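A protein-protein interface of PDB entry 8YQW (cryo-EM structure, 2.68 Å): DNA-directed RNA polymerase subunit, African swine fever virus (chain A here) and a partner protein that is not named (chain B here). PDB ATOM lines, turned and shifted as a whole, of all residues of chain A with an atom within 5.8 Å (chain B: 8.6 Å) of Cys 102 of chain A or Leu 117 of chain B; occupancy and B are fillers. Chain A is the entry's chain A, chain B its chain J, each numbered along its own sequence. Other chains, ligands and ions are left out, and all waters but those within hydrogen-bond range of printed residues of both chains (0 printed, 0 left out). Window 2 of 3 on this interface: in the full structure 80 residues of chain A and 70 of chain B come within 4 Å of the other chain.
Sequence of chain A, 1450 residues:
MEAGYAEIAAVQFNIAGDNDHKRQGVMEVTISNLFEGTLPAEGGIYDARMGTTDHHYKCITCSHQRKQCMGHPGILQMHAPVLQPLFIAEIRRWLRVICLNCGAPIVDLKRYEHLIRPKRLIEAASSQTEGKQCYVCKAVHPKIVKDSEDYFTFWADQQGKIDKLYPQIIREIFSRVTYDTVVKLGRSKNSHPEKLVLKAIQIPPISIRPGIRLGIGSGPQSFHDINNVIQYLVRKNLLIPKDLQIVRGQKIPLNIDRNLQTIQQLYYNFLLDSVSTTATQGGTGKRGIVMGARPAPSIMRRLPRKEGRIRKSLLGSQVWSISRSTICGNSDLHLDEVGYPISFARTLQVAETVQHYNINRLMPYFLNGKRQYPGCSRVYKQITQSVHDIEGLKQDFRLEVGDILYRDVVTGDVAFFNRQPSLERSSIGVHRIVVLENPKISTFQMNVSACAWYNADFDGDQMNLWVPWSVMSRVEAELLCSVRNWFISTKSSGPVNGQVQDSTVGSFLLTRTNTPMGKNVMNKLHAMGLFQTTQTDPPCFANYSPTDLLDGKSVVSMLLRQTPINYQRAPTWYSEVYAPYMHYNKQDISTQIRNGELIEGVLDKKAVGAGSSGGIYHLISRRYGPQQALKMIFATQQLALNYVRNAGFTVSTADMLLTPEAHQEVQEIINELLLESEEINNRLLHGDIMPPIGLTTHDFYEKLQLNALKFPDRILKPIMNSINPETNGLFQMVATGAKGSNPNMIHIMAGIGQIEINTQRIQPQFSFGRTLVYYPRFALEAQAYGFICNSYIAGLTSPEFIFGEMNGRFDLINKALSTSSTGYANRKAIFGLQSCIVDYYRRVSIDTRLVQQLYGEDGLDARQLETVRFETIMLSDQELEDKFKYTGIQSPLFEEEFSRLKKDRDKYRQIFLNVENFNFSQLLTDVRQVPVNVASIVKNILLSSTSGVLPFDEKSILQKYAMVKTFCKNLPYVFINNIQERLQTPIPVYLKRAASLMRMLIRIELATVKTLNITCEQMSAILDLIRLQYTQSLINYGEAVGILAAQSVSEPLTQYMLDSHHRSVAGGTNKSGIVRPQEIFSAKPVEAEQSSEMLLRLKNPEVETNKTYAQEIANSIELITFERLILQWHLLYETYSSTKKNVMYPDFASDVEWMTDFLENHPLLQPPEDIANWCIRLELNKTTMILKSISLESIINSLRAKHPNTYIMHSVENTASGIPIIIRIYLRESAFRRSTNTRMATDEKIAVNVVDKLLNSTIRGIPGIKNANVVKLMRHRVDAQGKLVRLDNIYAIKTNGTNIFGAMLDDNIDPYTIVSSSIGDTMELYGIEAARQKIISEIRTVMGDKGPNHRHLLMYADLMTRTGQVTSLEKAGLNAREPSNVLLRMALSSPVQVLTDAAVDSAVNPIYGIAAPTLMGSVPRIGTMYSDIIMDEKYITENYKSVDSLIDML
OE2 of Glu 108 of chain B is in salt-bridge range of NH2 of Arg 106 of chain B, at 3.3 Å. A ring nitrogen (NE2) of His 116 of chain B sits close to the side-chain carboxylate (OE1) of Glu 108 of chain B (3.3 Å). The backbone NH (N) of Ile 109 of chain B is in hydrogen-bond range of the backbone carbonyl oxygen (O) of Leu 117 of chain B, at 2.9 Å. The side-chain sulfur of Cys 102 of chain A lies close to the backbone NH of Ala 104 of chain A (3.5 Å). SG of Cys 134 of chain A lies close to N of Val 136 of chain A, at 3.7 Å. O of Asn 101 of chain A lies within hydrogen-bond range of NH1 of Arg 176 of chain A.
Among the printed residues, merely in contact across the chains: Arg 176 of chain A with Ala 118 of chain B (3.1 Å), Cys 102 of chain A with Leu 117 of chain B (3.5 Å), Thr 178 of chain A with Ala 118 of chain B (3.5 Å), Thr 178 of chain A with Glu 108 of chain B (3.8 Å), Thr 178 of chain A with Leu 117 of chain B (3.8 Å), Val 136 of chain A with Thr 115 of chain B (3.8 Å) and Arg 176 of chain A with Pro 120 of chain B (3.99 Å).
Printed residues of chain B that touch a printed residue of chain A: Glu 108, Thr 115, Leu 117, Ala 118 and Pro 120. Hydrophobic or aromatic side chains of chain B that line the printed part of chain A: Leu 117, Ala 118 and Pro 120. Of the 11 printed residues of chain A, 4 touch a printed residue of chain B. Printed residues of chain A that touch a printed residue of chain B: Cys 102, Val 136, Arg 176 and Thr 178. Among the printed residues, no Asp or Glu carboxylate lies within 4 Å of a Lys or Arg side-chain nitrogen of the other chain.
Cys 102 of chain A touches just one residue of chain B: Leu 117 (3.5 Å). Leu 117 of chain B touches just these residues of chain A: Cys 102 and Thr 178. Gly 103 of chain A touches none of the printed residues of chain B. Of the printed residues of chain B, Arg 176 of chain A touches Ala 118 (3.1 Å) and Pro 120 (3.99 Å). Printed residues of chain A within 4 Å of Thr 115 of chain B: Val 136 (3.8 Å). Of the printed residues of chain A, Pro 120 of chain B touches Arg 176. Of the printed residues of chain A, Ala 118 of chain B touches Arg 176 and Thr 178. Ile 125 of chain B touches none of the printed residues of chain A. Cys 134 of chain A touches none of the printed residues of chain B. The nearest residue of chain A that does not touch Leu 117 of chain B is Val 136 of chain A (4.7 Å). The nearest printed residue of chain A that does not touch Pro 120 of chain B is Cys 102 of chain A (7.5 Å).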
ATOM      1  N   CYS A  99     -13.382 -14.624  -4.807  1.00  0.00           N
ATOM      2  CA  CYS A  99     -13.736 -14.613  -6.217  1.00  0.00           C
ATOM      3  C   CYS A  99     -12.478 -14.601  -7.074  1.00  0.00           C
ATOM      4  O   CYS A  99     -11.523 -13.872  -6.794  1.00  0.00           O
ATOM      5  CB  CYS A  99     -14.605 -13.401  -6.539  1.00  0.00           C
ATOM      6  SG  CYS A  99     -15.067 -13.268  -8.277  1.00  0.00           S
ATOM      7  N   LEU A 100     -12.486 -15.406  -8.133  1.00  0.00           N
ATOM      8  CA  LEU A 100     -11.333 -15.539  -9.013  1.00  0.00           C
ATOM      9  C   LEU A 100     -11.232 -14.424 -10.042  1.00  0.00           C
ATOM     10  O   LEU A 100     -10.306 -14.442 -10.857  1.00  0.00           O
ATOM     11  CB  LEU A 100     -11.372 -16.890  -9.731  1.00  0.00           C
ATOM     12  CG  LEU A 100     -10.655 -18.060  -9.060  1.00  0.00           C
ATOM     13  CD1 LEU A 100     -11.288 -18.396  -7.726  1.00  0.00           C
ATOM     14  CD2 LEU A 100     -10.666 -19.270  -9.973  1.00  0.00           C
ATOM     15  N   ASN A 101     -12.153 -13.460 -10.030  1.00  0.00           N
ATOM     16  CA  ASN A 101     -12.169 -12.404 -11.030  1.00  0.00           C
ATOM     17  C   ASN A 101     -12.049 -11.001 -10.454  1.00  0.00           C
ATOM     18  O   ASN A 101     -11.516 -10.122 -11.139  1.00  0.00           O
ATOM     19  CB  ASN A 101     -13.452 -12.487 -11.871  1.00  0.00           C
ATOM     20  CG  ASN A 101     -13.321 -11.787 -13.207  1.00  0.00           C
ATOM     21  OD1 ASN A 101     -12.258 -11.273 -13.552  1.00  0.00           O
ATOM     22  ND2 ASN A 101     -14.406 -11.767 -13.970  1.00  0.00           N
ATOM     23  N   CYS A 102     -12.519 -10.760  -9.229  1.00  0.00           N
ATOM     24  CA  CYS A 102     -12.389  -9.448  -8.610  1.00  0.00           C
ATOM     25  C   CYS A 102     -11.715  -9.470  -7.247  1.00  0.00           C
ATOM     26  O   CYS A 102     -11.390  -8.396  -6.729  1.00  0.00           O
ATOM     27  CB  CYS A 102     -13.763  -8.778  -8.465  1.00  0.00           C
ATOM     28  SG  CYS A 102     -14.842  -9.580  -7.278  1.00  0.00           S
ATOM     29  N   GLY A 103     -11.497 -10.639  -6.651  1.00  0.00           N
ATOM     30  CA  GLY A 103     -10.819 -10.737  -5.379  1.00  0.00           C
ATOM     31  C   GLY A 103     -11.699 -10.572  -4.161  1.00  0.00           C
ATOM     32  O   GLY A 103     -11.207 -10.730  -3.038  1.00  0.00           O
ATOM     33  N   ALA A 104     -12.976 -10.260  -4.341  1.00  0.00           N
ATOM     34  CA  ALA A 104     -13.879 -10.102  -3.216  1.00  0.00           C
ATOM     35  C   ALA A 104     -14.261 -11.465  -2.640  1.00  0.00           C
ATOM     36  O   ALA A 104     -14.212 -12.478  -3.342  1.00  0.00           O
ATOM     37  CB  ALA A 104     -15.133  -9.353  -3.648  1.00  0.00           C
ATOM     38  N   CYS A 134     -21.016 -13.932  -7.463  1.00  0.00           N
ATOM     39  CA  CYS A 134     -20.357 -12.819  -6.799  1.00  0.00           C
ATOM     40  C   CYS A 134     -21.303 -11.630  -6.668  1.00  0.00           C
ATOM     41  O   CYS A 134     -22.206 -11.432  -7.486  1.00  0.00           O
ATOM     42  CB  CYS A 134     -19.103 -12.411  -7.569  1.00  0.00           C
ATOM     43  SG  CYS A 134     -17.996 -11.324  -6.657  1.00  0.00           S
ATOM     44  N   VAL A 136     -20.244  -8.344  -6.474  1.00  0.00           N
ATOM     45  CA  VAL A 136     -19.682  -7.087  -6.960  1.00  0.00           C
ATOM     46  C   VAL A 136     -19.201  -7.149  -8.399  1.00  0.00           C
ATOM     47  O   VAL A 136     -19.089  -6.093  -9.049  1.00  0.00           O
ATOM     48  CB  VAL A 136     -18.537  -6.615  -6.036  1.00  0.00           C
ATOM     49  CG1 VAL A 136     -19.090  -6.148  -4.701  1.00  0.00           C
ATOM     50  CG2 VAL A 136     -17.535  -7.728  -5.832  1.00  0.00           C
ATOM     51  N   CYS A 137     -18.899  -8.320  -8.956  1.00  0.00           N
ATOM     52  CA  CYS A 137     -18.459  -8.419 -10.338  1.00  0.00           C
ATOM     53  C   CYS A 137     -19.317  -9.343 -11.187  1.00  0.00           C
ATOM     54  O   CYS A 137     -19.103  -9.405 -12.405  1.00  0.00           O
ATOM     55  CB  CYS A 137     -17.001  -8.899 -10.407  1.00  0.00           C
ATOM     56  SG  CYS A 137     -16.821 -10.687 -10.316  1.00  0.00           S
ATOM     57  N   ARG A 176      -5.295  -9.637  -5.525  1.00  0.00           N
ATOM     58  CA  ARG A 176      -6.520  -8.860  -5.572  1.00  0.00           C
ATOM     59  C   ARG A 176      -7.314  -8.951  -4.274  1.00  0.00           C
ATOM     60  O   ARG A 176      -8.399  -8.367  -4.182  1.00  0.00           O
ATOM     61  CB  ARG A 176      -7.367  -9.327  -6.761  1.00  0.00           C
ATOM     62  CG  ARG A 176      -8.205  -8.244  -7.392  1.00  0.00           C
ATOM     63  CD  ARG A 176      -8.837  -8.698  -8.696  1.00  0.00           C
ATOM     64  NE  ARG A 176      -7.862  -9.092  -9.703  1.00  0.00           N
ATOM     65  CZ  ARG A 176      -7.841 -10.277 -10.295  1.00  0.00           C
ATOM     66  NH1 ARG A 176      -8.716 -11.219  -9.987  1.00  0.00           N
ATOM     67  NH2 ARG A 176      -6.919 -10.524 -11.222  1.00  0.00           N
ATOM     68  N   THR A 178      -7.994  -8.049  -0.388  1.00  0.00           N
ATOM     69  CA  THR A 178      -7.689  -6.955   0.515  1.00  0.00           C
ATOM     70  C   THR A 178      -7.328  -7.488   1.899  1.00  0.00           C
ATOM     71  O   THR A 178      -7.636  -8.627   2.255  1.00  0.00           O
ATOM     72  CB  THR A 178      -8.871  -5.991   0.613  1.00  0.00           C
ATOM     73  OG1 THR A 178      -9.996  -6.668   1.187  1.00  0.00           O
ATOM     74  CG2 THR A 178      -9.249  -5.480  -0.765  1.00  0.00           C
ATOM     75  N   PRO B  90      -5.787   5.699  -0.373  1.00  0.00           N
ATOM     76  CA  PRO B  90      -6.478   4.885  -1.375  1.00  0.00           C
ATOM     77  C   PRO B  90      -7.216   5.769  -2.366  1.00  0.00           C
ATOM     78  O   PRO B  90      -7.462   6.951  -2.118  1.00  0.00           O
ATOM     79  CB  PRO B  90      -7.448   4.060  -0.523  1.00  0.00           C
ATOM     80  CG  PRO B  90      -7.793   5.041   0.560  1.00  0.00           C
ATOM     81  CD  PRO B  90      -6.403   5.492   0.949  1.00  0.00           C
ATOM     82  N   ILE B  91      -7.573   5.181  -3.502  1.00  0.00           N
ATOM     83  CA  ILE B  91      -8.152   5.924  -4.613  1.00  0.00           C
ATOM     84  C   ILE B  91      -9.554   5.398  -4.893  1.00  0.00           C
ATOM     85  O   ILE B  91      -9.869   4.233  -4.626  1.00  0.00           O
ATOM     86  CB  ILE B  91      -7.259   5.827  -5.870  1.00  0.00           C
ATOM     87  CG1 ILE B  91      -5.812   6.185  -5.530  1.00  0.00           C
ATOM     88  CG2 ILE B  91      -7.751   6.758  -6.953  1.00  0.00           C
ATOM     89  CD1 ILE B  91      -4.915   4.991  -5.299  1.00  0.00           C
ATOM     90  N   SER B  93     -12.502   4.843  -7.868  1.00  0.00           N
ATOM     91  CA  SER B  93     -12.525   4.554  -9.293  1.00  0.00           C
ATOM     92  C   SER B  93     -13.948   4.595  -9.832  1.00  0.00           C
ATOM     93  O   SER B  93     -14.871   4.043  -9.225  1.00  0.00           O
ATOM     94  CB  SER B  93     -11.900   3.186  -9.579  1.00  0.00           C
ATOM     95  OG  SER B  93     -12.654   2.146  -8.983  1.00  0.00           O
ATOM     96  N   ARG B 106       0.419  -3.790  -6.151  1.00  0.00           N
ATOM     97  CA  ARG B 106      -0.980  -4.022  -5.822  1.00  0.00           C
ATOM     98  C   ARG B 106      -1.478  -2.908  -4.914  1.00  0.00           C
ATOM     99  O   ARG B 106      -0.794  -2.494  -3.973  1.00  0.00           O
ATOM    100  CB  ARG B 106      -1.165  -5.391  -5.159  1.00  0.00           C
ATOM    101  CG  ARG B 106      -0.579  -5.515  -3.766  1.00  0.00           C
ATOM    102  CD  ARG B 106      -1.101  -6.743  -3.042  1.00  0.00           C
ATOM    103  NE  ARG B 106      -2.487  -6.593  -2.614  1.00  0.00           N
ATOM    104  CZ  ARG B 106      -2.875  -5.879  -1.565  1.00  0.00           C
ATOM    105  NH1 ARG B 106      -2.006  -5.208  -0.827  1.00  0.00           N
ATOM    106  NH2 ARG B 106      -4.165  -5.840  -1.248  1.00  0.00           N
ATOM    107  N   LYS B 107      -2.661  -2.388  -5.221  1.00  0.00           N
ATOM    108  CA  LYS B 107      -3.195  -1.239  -4.505  1.00  0.00           C
ATOM    109  C   LYS B 107      -4.635  -1.514  -4.108  1.00  0.00           C
ATOM    110  O   LYS B 107      -5.425  -1.993  -4.926  1.00  0.00           O
ATOM    111  CB  LYS B 107      -3.112   0.031  -5.358  1.00  0.00           C
ATOM    112  CG  LYS B 107      -3.604   1.280  -4.651  1.00  0.00           C
ATOM    113  CD  LYS B 107      -2.716   1.619  -3.469  1.00  0.00           C
ATOM    114  CE  LYS B 107      -3.104   2.946  -2.846  1.00  0.00           C
ATOM    115  NZ  LYS B 107      -2.286   3.246  -1.642  1.00  0.00           N
ATOM    116  N   GLU B 108      -4.971  -1.219  -2.857  1.00  0.00           N
ATOM    117  CA  GLU B 108      -6.344  -1.325  -2.384  1.00  0.00           C
ATOM    118  C   GLU B 108      -7.057  -0.011  -2.667  1.00  0.00           C
ATOM    119  O   GLU B 108      -6.726   1.020  -2.074  1.00  0.00           O
ATOM    120  CB  GLU B 108      -6.384  -1.658  -0.894  1.00  0.00           C
ATOM    121  CG  GLU B 108      -5.655  -2.934  -0.527  1.00  0.00           C
ATOM    122  CD  GLU B 108      -5.918  -3.365   0.902  1.00  0.00           C
ATOM    123  OE1 GLU B 108      -6.845  -2.814   1.531  1.00  0.00           O
ATOM    124  OE2 GLU B 108      -5.198  -4.255   1.396  1.00  0.00           O
ATOM    125  N   ILE B 109      -8.028  -0.048  -3.576  1.00  0.00           N
ATOM    126  CA  ILE B 109      -8.755   1.135  -4.001  1.00  0.00           C
ATOM    127  C   ILE B 109     -10.228   0.960  -3.651  1.00  0.00           C
ATOM    128  O   ILE B 109     -10.684  -0.120  -3.261  1.00  0.00           O
ATOM    129  CB  ILE B 109      -8.584   1.419  -5.506  1.00  0.00           C
ATOM    130  CG1 ILE B 109      -9.207   0.294  -6.333  1.00  0.00           C
ATOM    131  CG2 ILE B 109      -7.117   1.584  -5.857  1.00  0.00           C
ATOM    132  CD1 ILE B 109      -9.751   0.753  -7.667  1.00  0.00           C
ATOM    133  N   PHE B 110     -10.963   2.056  -3.784  1.00  0.00           N
ATOM    134  CA  PHE B 110     -12.393   2.094  -3.543  1.00  0.00           C
ATOM    135  C   PHE B 110     -13.115   2.380  -4.850  1.00  0.00           C
ATOM    136  O   PHE B 110     -12.522   2.837  -5.830  1.00  0.00           O
ATOM    137  CB  PHE B 110     -12.754   3.160  -2.502  1.00  0.00           C
ATOM    138  CG  PHE B 110     -12.594   2.705  -1.081  1.00  0.00           C
ATOM    139  CD1 PHE B 110     -13.579   1.952  -0.465  1.00  0.00           C
ATOM    140  CD2 PHE B 110     -11.463   3.039  -0.357  1.00  0.00           C
ATOM    141  CE1 PHE B 110     -13.431   1.533   0.844  1.00  0.00           C
ATOM    142  CE2 PHE B 110     -11.311   2.627   0.950  1.00  0.00           C
ATOM    143  CZ  PHE B 110     -12.297   1.872   1.552  1.00  0.00           C
ATOM    144  N   LEU B 111     -14.410   2.092  -4.858  1.00  0.00           N
ATOM    145  CA  LEU B 111     -15.273   2.412  -5.982  1.00  0.00           C
ATOM    146  C   LEU B 111     -16.308   3.436  -5.540  1.00  0.00           C
ATOM    147  O   LEU B 111     -16.588   3.590  -4.348  1.00  0.00           O
ATOM    148  CB  LEU B 111     -15.977   1.161  -6.528  1.00  0.00           C
ATOM    149  CG  LEU B 111     -15.145   0.188  -7.365  1.00  0.00           C
ATOM    150  CD1 LEU B 111     -14.427  -0.810  -6.476  1.00  0.00           C
ATOM    151  CD2 LEU B 111     -16.016  -0.530  -8.380  1.00  0.00           C
ATOM    152  N   ASN B 113     -19.944   4.453  -4.830  1.00  0.00           N
ATOM    153  CA  ASN B 113     -20.897   3.727  -3.974  1.00  0.00           C
ATOM    154  C   ASN B 113     -20.173   2.979  -2.858  1.00  0.00           C
ATOM    155  O   ASN B 113     -20.816   2.212  -2.132  1.00  0.00           O
ATOM    156  CB  ASN B 113     -21.845   2.765  -4.725  1.00  0.00           C
ATOM    157  CG  ASN B 113     -21.205   1.424  -5.128  1.00  0.00           C
ATOM    158  OD1 ASN B 113     -20.080   1.091  -4.760  1.00  0.00           O
ATOM    159  ND2 ASN B 113     -21.949   0.653  -5.913  1.00  0.00           N
ATOM    160  N   GLY B 114     -18.866   3.172  -2.697  1.00  0.00           N
ATOM    161  CA  GLY B 114     -18.155   2.674  -1.534  1.00  0.00           C
ATOM    162  C   GLY B 114     -17.987   1.172  -1.448  1.00  0.00           C
ATOM    163  O   GLY B 114     -18.581   0.528  -0.579  1.00  0.00           O
ATOM    164  N   THR B 115     -17.183   0.598  -2.339  1.00  0.00           N
ATOM    165  CA  THR B 115     -16.815  -0.809  -2.274  1.00  0.00           C
ATOM    166  C   THR B 115     -15.300  -0.916  -2.366  1.00  0.00           C
ATOM    167  O   THR B 115     -14.682  -0.272  -3.219  1.00  0.00           O
ATOM    168  CB  THR B 115     -17.484  -1.615  -3.390  1.00  0.00           C
ATOM    169  OG1 THR B 115     -18.867  -1.258  -3.472  1.00  0.00           O
ATOM    170  CG2 THR B 115     -17.385  -3.100  -3.096  1.00  0.00           C
ATOM    171  N   HIS B 116     -14.709  -1.729  -1.493  1.00  0.00           N
ATOM    172  CA  HIS B 116     -13.262  -1.816  -1.338  1.00  0.00           C
ATOM    173  C   HIS B 116     -12.740  -3.045  -2.072  1.00  0.00           C
ATOM    174  O   HIS B 116     -13.105  -4.175  -1.732  1.00  0.00           O
ATOM    175  CB  HIS B 116     -12.897  -1.886   0.145  1.00  0.00           C
ATOM    176  CG  HIS B 116     -11.458  -1.596   0.434  1.00  0.00           C
ATOM    177  ND1 HIS B 116     -10.860  -1.929   1.629  1.00  0.00           N
ATOM    178  CD2 HIS B 116     -10.499  -1.001  -0.313  1.00  0.00           C
ATOM    179  CE1 HIS B 116      -9.595  -1.553   1.606  1.00  0.00           C
ATOM    180  NE2 HIS B 116      -9.350  -0.987   0.438  1.00  0.00           N
ATOM    181  N   LEU B 117     -11.880  -2.827  -3.068  1.00  0.00           N
ATOM    182  CA  LEU B 117     -11.290  -3.925  -3.819  1.00  0.00           C
ATOM    183  C   LEU B 117      -9.821  -3.631  -4.071  1.00  0.00           C
ATOM    184  O   LEU B 117      -9.414  -2.473  -4.165  1.00  0.00           O
ATOM    185  CB  LEU B 117     -11.999  -4.163  -5.163  1.00  0.00           C
ATOM    186  CG  LEU B 117     -13.214  -5.092  -5.206  1.00  0.00           C
ATOM    187  CD1 LEU B 117     -14.459  -4.401  -4.692  1.00  0.00           C
ATOM    188  CD2 LEU B 117     -13.435  -5.606  -6.618  1.00  0.00           C
ATOM    189  N   ALA B 118      -9.030  -4.687  -4.194  1.00  0.00           N
ATOM    190  CA  ALA B 118      -7.622  -4.547  -4.525  1.00  0.00           C
ATOM    191  C   ALA B 118      -7.422  -4.726  -6.023  1.00  0.00           C
ATOM    192  O   ALA B 118      -8.282  -5.267  -6.722  1.00  0.00           O
ATOM    193  CB  ALA B 118      -6.774  -5.560  -3.757  1.00  0.00           C
ATOM    194  N   VAL B 119      -6.291  -4.236  -6.517  1.00  0.00           N
ATOM    195  CA  VAL B 119      -5.910  -4.438  -7.912  1.00  0.00           C
ATOM    196  C   VAL B 119      -4.448  -4.866  -7.954  1.00  0.00           C
ATOM    197  O   VAL B 119      -3.642  -4.412  -7.127  1.00  0.00           O
ATOM    198  CB  VAL B 119      -6.149  -3.175  -8.758  1.00  0.00           C
ATOM    199  CG1 VAL B 119      -7.637  -2.951  -8.974  1.00  0.00           C
ATOM    200  CG2 VAL B 119      -5.517  -1.961  -8.106  1.00  0.00           C
ATOM    201  N   PRO B 120      -4.062  -5.726  -8.904  1.00  0.00           N
ATOM    202  CA  PRO B 120      -2.675  -6.209  -8.952  1.00  0.00           C
ATOM    203  C   PRO B 120      -1.673  -5.131  -9.332  1.00  0.00           C
ATOM    204  O   PRO B 120      -2.029  -3.961  -9.500  1.00  0.00           O
ATOM    205  CB  PRO B 120      -2.726  -7.322 -10.008  1.00  0.00           C
ATOM    206  CG  PRO B 120      -3.938  -7.028 -10.823  1.00  0.00           C
ATOM    207  CD  PRO B 120      -4.922  -6.407  -9.885  1.00  0.00           C
ATOM    208  N   ILE B 125      -6.478   1.647 -13.769  1.00  0.00           N
ATOM    209  CA  ILE B 125      -7.533   2.159 -12.906  1.00  0.00           C
ATOM    210  C   ILE B 125      -7.699   3.645 -13.185  1.00  0.00           C
ATOM    211  O   ILE B 125      -6.711   4.364 -13.375  1.00  0.00           O
ATOM    212  CB  ILE B 125      -7.237   1.902 -11.415  1.00  0.00           C
ATOM    213  CG1 ILE B 125      -5.877   2.480 -11.021  1.00  0.00           C
ATOM    214  CG2 ILE B 125      -7.306   0.415 -11.109  1.00  0.00           C
ATOM    215  CD1 ILE B 125      -5.615   2.475  -9.534  1.00  0.00           C
